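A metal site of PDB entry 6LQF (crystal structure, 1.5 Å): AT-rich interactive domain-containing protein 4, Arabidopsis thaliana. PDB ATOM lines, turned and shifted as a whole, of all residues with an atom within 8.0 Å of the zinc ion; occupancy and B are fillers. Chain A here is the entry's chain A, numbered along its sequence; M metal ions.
The side-chain sulfur (SG) of Cys 16 sits close to the backbone NH (N) of Arg 18 (3.5 Å). A ring nitrogen (NE2) of His 14 lies within hydrogen-bond range of the side-chain amide nitrogen (NE2) of Gln 35 (3.4 Å). A ring nitrogen (ND1) of His 126 lies within hydrogen-bond range of the backbone carbonyl oxygen of Tyr 122. The backbone carbonyl oxygen (O) of His 126 lies within hydrogen-bond range of the side-chain amino group (NZ) of Lys 13, 2.8 Å away. The backbone NH (N) of His 14 lies within hydrogen-bond range of the backbone carbonyl oxygen (O) of Ala 125. The side-chain hydroxyl (OH) of Tyr 122 lies within hydrogen-bond range of the guanidinium group (NH1) of Arg 18, at 2.9 Å. The side-chain carboxylate (OD2) of Asp 32 lies close to the side-chain hydroxyl (OH) of Tyr 122, 2.7 Å away.
Tyr 122 touches the zinc ion (OH to ZN, 3.97 Å). Five residues have an atom within 4 Å of the zinc ion: His 14, Cys 16, Asp 32, Tyr 122 and His 126. The nearest printed residue that does not touch the zinc ion is Arg 18 (4.5 Å).
The zinc ion is bound by a ring nitrogen (NE2) of His 126 (2.0 Å), a ring nitrogen (ND1) of His 14 (2.1 Å), the side-chain carboxylate of Asp 32 (2.1 Å) and the side-chain sulfur of Cys 16 (2.2 Å). The zinc ion has four donor atoms within binding distance.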
ATOM      1  N   LYS A  13      18.340  24.381  22.754  1.00  0.00           N
ATOM      2  CA  LYS A  13      19.306  25.481  22.912  1.00  0.00           C
ATOM      3  C   LYS A  13      19.332  26.016  24.345  1.00  0.00           C
ATOM      4  O   LYS A  13      18.330  25.996  25.054  1.00  0.00           O
ATOM      5  CB  LYS A  13      19.008  26.638  21.946  1.00  0.00           C
ATOM      6  CG  LYS A  13      19.041  26.285  20.437  1.00  0.00           C
ATOM      7  CD  LYS A  13      20.417  25.854  19.989  1.00  0.00           C
ATOM      8  CE  LYS A  13      20.410  25.227  18.607  1.00  0.00           C
ATOM      9  NZ  LYS A  13      21.813  24.895  18.175  1.00  0.00           N
ATOM     10  N   HIS A  14      20.510  26.463  24.771  1.00  0.00           N
ATOM     11  CA  HIS A  14      20.711  27.124  26.056  1.00  0.00           C
ATOM     12  C   HIS A  14      19.994  28.469  26.021  1.00  0.00           C
ATOM     13  O   HIS A  14      20.032  29.137  24.995  1.00  0.00           O
ATOM     14  CB  HIS A  14      22.213  27.327  26.273  1.00  0.00           C
ATOM     15  CG  HIS A  14      22.605  27.563  27.691  1.00  0.00           C
ATOM     16  ND1 HIS A  14      23.713  28.303  28.034  1.00  0.00           N
ATOM     17  CD2 HIS A  14      22.064  27.119  28.842  1.00  0.00           C
ATOM     18  CE1 HIS A  14      23.834  28.305  29.348  1.00  0.00           C
ATOM     19  NE2 HIS A  14      22.856  27.590  29.866  1.00  0.00           N
ATOM     20  N   ASP A  15      19.351  28.938  27.082  1.00  0.00           N
ATOM     21  CA  ASP A  15      18.803  30.280  26.830  1.00  0.00           C
ATOM     22  C   ASP A  15      19.887  31.351  27.028  1.00  0.00           C
ATOM     23  O   ASP A  15      20.288  31.987  26.071  1.00  0.00           O
ATOM     24  CB  ASP A  15      17.548  30.551  27.647  1.00  0.00           C
ATOM     25  CG  ASP A  15      16.303  30.491  26.762  1.00  0.00           C
ATOM     26  OD1 ASP A  15      16.414  29.889  25.665  1.00  0.00           O
ATOM     27  OD2 ASP A  15      15.240  31.012  27.146  1.00  0.00           O
ATOM     28  N   CYS A  16      20.349  31.518  28.250  1.00  0.00           N
ATOM     29  CA  CYS A  16      21.571  32.279  28.511  1.00  0.00           C
ATOM     30  C   CYS A  16      21.653  33.702  27.925  1.00  0.00           C
ATOM     31  O   CYS A  16      22.016  34.621  28.643  1.00  0.00           O
ATOM     32  CB  CYS A  16      22.808  31.455  28.078  1.00  0.00           C
ATOM     33  SG  CYS A  16      23.317  31.283  26.318  1.00  0.00           S
ATOM     34  N   GLY A  17      21.336  33.915  26.662  1.00  0.00           N
ATOM     35  CA  GLY A  17      21.550  35.236  26.063  1.00  0.00           C
ATOM     36  C   GLY A  17      23.002  35.704  25.979  1.00  0.00           C
ATOM     37  O   GLY A  17      23.279  36.905  25.946  1.00  0.00           O
ATOM     38  N   ARG A  18      23.924  34.753  25.968  1.00  0.00           N
ATOM     39  CA  ARG A  18      25.353  35.022  25.826  1.00  0.00           C
ATOM     40  C   ARG A  18      25.600  35.786  24.546  1.00  0.00           C
ATOM     41  O   ARG A  18      24.909  35.554  23.533  1.00  0.00           O
ATOM     42  CB  ARG A  18      26.123  33.703  25.793  1.00  0.00           C
ATOM     43  CG  ARG A  18      27.636  33.794  26.084  1.00  0.00           C
ATOM     44  CD  ARG A  18      28.377  32.767  25.280  1.00  0.00           C
ATOM     45  NE  ARG A  18      28.265  33.099  23.861  1.00  0.00           N
ATOM     46  CZ  ARG A  18      28.248  32.218  22.874  1.00  0.00           C
ATOM     47  NH1 ARG A  18      28.326  30.907  23.116  1.00  0.00           N
ATOM     48  NH2 ARG A  18      28.151  32.672  21.599  1.00  0.00           N
ATOM     49  N   ALA A  19      26.576  36.688  24.574  1.00  0.00           N
ATOM     50  CA  ALA A  19      26.980  37.446  23.395  1.00  0.00           C
ATOM     51  C   ALA A  19      27.311  36.523  22.203  1.00  0.00           C
ATOM     52  O   ALA A  19      27.813  35.427  22.401  1.00  0.00           O
ATOM     53  CB  ALA A  19      28.192  38.318  23.703  1.00  0.00           C
ATOM     54  N   GLU A  28      32.948  35.969  29.757  1.00  0.00           N
ATOM     55  CA  GLU A  28      31.540  35.701  29.527  1.00  0.00           C
ATOM     56  C   GLU A  28      31.316  34.306  28.943  1.00  0.00           C
ATOM     57  O   GLU A  28      30.410  33.585  29.370  1.00  0.00           O
ATOM     58  CB  GLU A  28      30.939  36.739  28.580  1.00  0.00           C
ATOM     59  CG  GLU A  28      29.462  36.517  28.381  1.00  0.00           C
ATOM     60  CD  GLU A  28      28.769  37.594  27.546  1.00  0.00           C
ATOM     61  OE1 GLU A  28      29.355  38.681  27.338  1.00  0.00           O
ATOM     62  OE2 GLU A  28      27.615  37.349  27.148  1.00  0.00           O
ATOM     63  N   PHE A  29      32.164  33.895  27.985  1.00  0.00           N
ATOM     64  CA  PHE A  29      32.066  32.549  27.443  1.00  0.00           C
ATOM     65  C   PHE A  29      32.270  31.479  28.520  1.00  0.00           C
ATOM     66  O   PHE A  29      31.439  30.564  28.643  1.00  0.00           O
ATOM     67  CB  PHE A  29      33.101  32.379  26.313  1.00  0.00           C
ATOM     68  CG  PHE A  29      33.191  30.991  25.828  1.00  0.00           C
ATOM     69  CD1 PHE A  29      32.247  30.514  24.909  1.00  0.00           C
ATOM     70  CD2 PHE A  29      34.196  30.144  26.252  1.00  0.00           C
ATOM     71  CE1 PHE A  29      32.297  29.161  24.455  1.00  0.00           C
ATOM     72  CE2 PHE A  29      34.247  28.795  25.766  1.00  0.00           C
ATOM     73  CZ  PHE A  29      33.300  28.339  24.878  1.00  0.00           C
ATOM     74  N   ARG A  31      32.072  31.561  31.750  1.00  0.00           N
ATOM     75  CA  ARG A  31      31.016  31.507  32.755  1.00  0.00           C
ATOM     76  C   ARG A  31      29.788  30.845  32.183  1.00  0.00           C
ATOM     77  O   ARG A  31      29.117  30.066  32.901  1.00  0.00           O
ATOM     78  CB  ARG A  31      30.731  32.918  33.296  1.00  0.00           C
ATOM     79  CG  ARG A  31      31.898  33.446  34.131  1.00  0.00           C
ATOM     80  CD  ARG A  31      31.492  34.735  34.818  1.00  0.00           C
ATOM     81  NE  ARG A  31      32.595  35.291  35.578  1.00  0.00           N
ATOM     82  CZ  ARG A  31      32.903  34.914  36.822  1.00  0.00           C
ATOM     83  NH1 ARG A  31      32.188  33.962  37.423  1.00  0.00           N
ATOM     84  NH2 ARG A  31      33.945  35.451  37.452  1.00  0.00           N
ATOM     85  N   ASP A  32      29.500  31.080  30.902  1.00  0.00           N
ATOM     86  CA  ASP A  32      28.343  30.410  30.293  1.00  0.00           C
ATOM     87  C   ASP A  32      28.600  28.895  30.145  1.00  0.00           C
ATOM     88  O   ASP A  32      27.666  28.074  30.347  1.00  0.00           O
ATOM     89  CB  ASP A  32      27.989  31.031  28.928  1.00  0.00           C
ATOM     90  CG  ASP A  32      26.645  30.681  28.484  1.00  0.00           C
ATOM     91  OD1 ASP A  32      25.647  30.922  29.187  1.00  0.00           O
ATOM     92  OD2 ASP A  32      26.562  30.133  27.379  1.00  0.00           O
ATOM     93  N   VAL A  33      29.829  28.499  29.832  1.00  0.00           N
ATOM     94  CA  VAL A  33      30.146  27.060  29.770  1.00  0.00           C
ATOM     95  C   VAL A  33      29.974  26.404  31.133  1.00  0.00           C
ATOM     96  O   VAL A  33      29.380  25.297  31.221  1.00  0.00           O
ATOM     97  CB  VAL A  33      31.580  26.781  29.234  1.00  0.00           C
ATOM     98  CG1 VAL A  33      31.908  25.313  29.316  1.00  0.00           C
ATOM     99  CG2 VAL A  33      31.690  27.218  27.765  1.00  0.00           C
ATOM    100  N   GLN A  35      28.017  27.349  33.589  1.00  0.00           N
ATOM    101  CA  GLN A  35      26.597  27.273  33.949  1.00  0.00           C
ATOM    102  C   GLN A  35      25.913  26.131  33.190  1.00  0.00           C
ATOM    103  O   GLN A  35      25.108  25.365  33.725  1.00  0.00           O
ATOM    104  CB  GLN A  35      25.900  28.590  33.673  1.00  0.00           C
ATOM    105  CG  GLN A  35      24.437  28.595  34.118  1.00  0.00           C
ATOM    106  CD  GLN A  35      23.613  29.638  33.401  1.00  0.00           C
ATOM    107  OE1 GLN A  35      23.986  30.811  33.349  1.00  0.00           O
ATOM    108  NE2 GLN A  35      22.509  29.216  32.822  1.00  0.00           N
ATOM    109  N   PHE A  36      26.292  25.982  31.928  1.00  0.00           N
ATOM    110  CA  PHE A  36      25.728  24.930  31.062  1.00  0.00           C
ATOM    111  C   PHE A  36      26.107  23.564  31.584  1.00  0.00           C
ATOM    112  O   PHE A  36      25.272  22.667  31.648  1.00  0.00           O
ATOM    113  CB  PHE A  36      26.240  25.100  29.608  1.00  0.00           C
ATOM    114  CG  PHE A  36      25.764  24.027  28.692  1.00  0.00           C
ATOM    115  CD1 PHE A  36      24.508  24.105  28.153  1.00  0.00           C
ATOM    116  CD2 PHE A  36      26.587  22.934  28.381  1.00  0.00           C
ATOM    117  CE1 PHE A  36      24.030  23.083  27.326  1.00  0.00           C
ATOM    118  CE2 PHE A  36      26.119  21.937  27.544  1.00  0.00           C
ATOM    119  CZ  PHE A  36      24.857  22.026  27.009  1.00  0.00           C
ATOM    120  N   TYR A 122      27.766  21.611  24.635  1.00  0.00           N
ATOM    121  CA  TYR A 122      27.643  23.083  24.555  1.00  0.00           C
ATOM    122  C   TYR A 122      27.491  23.564  23.128  1.00  0.00           C
ATOM    123  O   TYR A 122      26.644  24.402  22.837  1.00  0.00           O
ATOM    124  CB  TYR A 122      28.841  23.750  25.235  1.00  0.00           C
ATOM    125  CG  TYR A 122      28.735  25.267  25.333  1.00  0.00           C
ATOM    126  CD1 TYR A 122      29.178  26.095  24.268  1.00  0.00           C
ATOM    127  CD2 TYR A 122      28.249  25.866  26.488  1.00  0.00           C
ATOM    128  CE1 TYR A 122      29.071  27.440  24.333  1.00  0.00           C
ATOM    129  CE2 TYR A 122      28.157  27.249  26.606  1.00  0.00           C
ATOM    130  CZ  TYR A 122      28.553  28.013  25.516  1.00  0.00           C
ATOM    131  OH  TYR A 122      28.456  29.384  25.595  1.00  0.00           O
ATOM    132  N   ALA A 125      24.072  23.055  21.851  1.00  0.00           N
ATOM    133  CA  ALA A 125      23.061  23.936  22.468  1.00  0.00           C
ATOM    134  C   ALA A 125      23.231  25.419  22.166  1.00  0.00           C
ATOM    135  O   ALA A 125      22.492  26.257  22.710  1.00  0.00           O
ATOM    136  CB  ALA A 125      23.069  23.752  23.980  1.00  0.00           C
ATOM    137  N   HIS A 126      24.187  25.770  21.307  1.00  0.00           N
ATOM    138  CA  HIS A 126      24.381  27.175  20.930  1.00  0.00           C
ATOM    139  C   HIS A 126      24.373  27.331  19.428  1.00  0.00           C
ATOM    140  O   HIS A 126      24.173  26.335  18.714  1.00  0.00           O
ATOM    141  CB  HIS A 126      25.652  27.726  21.571  1.00  0.00           C
ATOM    142  CG  HIS A 126      25.534  27.857  23.046  1.00  0.00           C
ATOM    143  ND1 HIS A 126      25.668  26.774  23.896  1.00  0.00           N
ATOM    144  CD2 HIS A 126      25.199  28.910  23.818  1.00  0.00           C
ATOM    145  CE1 HIS A 126      25.437  27.172  25.138  1.00  0.00           C
ATOM    146  NE2 HIS A 126      25.135  28.456  25.122  1.00  0.00           N
ATOM    147  N   ASP A 127      24.501  28.567  18.944  1.00  0.00           N
ATOM    148  CA  ASP A 127      24.381  28.820  17.499  1.00  0.00           C
ATOM    149  C   ASP A 127      25.624  29.501  17.010  1.00  0.00           C
ATOM    150  O   ASP A 127      25.568  30.534  16.317  1.00  0.00           O
ATOM    151  CB  ASP A 127      23.146  29.653  17.207  1.00  0.00           C
ATOM    152  CG  ASP A 127      21.876  28.931  17.585  1.00  0.00           C
ATOM    153  OD1 ASP A 127      21.649  27.808  17.075  1.00  0.00           O
ATOM    154  OD2 ASP A 127      21.125  29.484  18.422  1.00  0.00           O
ATOM    155  N   ASP A 128      26.765  28.897  17.320  1.00  0.00           N
ATOM    156  CA  ASP A 128      28.042  29.498  17.034  1.00  0.00           C
ATOM    157  C   ASP A 128      28.767  28.908  15.845  1.00  0.00           C
ATOM    158  O   ASP A 128      29.852  29.395  15.488  1.00  0.00           O
ATOM    159  CB  ASP A 128      28.933  29.357  18.258  1.00  0.00           C
ATOM    160  CG  ASP A 128      28.315  29.946  19.509  1.00  0.00           C
ATOM    161  OD1 ASP A 128      27.676  31.021  19.412  1.00  0.00           O
ATOM    162  OD2 ASP A 128      28.515  29.370  20.571  1.00  0.00           O
HETATM  163 ZN    ZN M   1      24.664  29.596  26.739  1.00  0.00          ZN
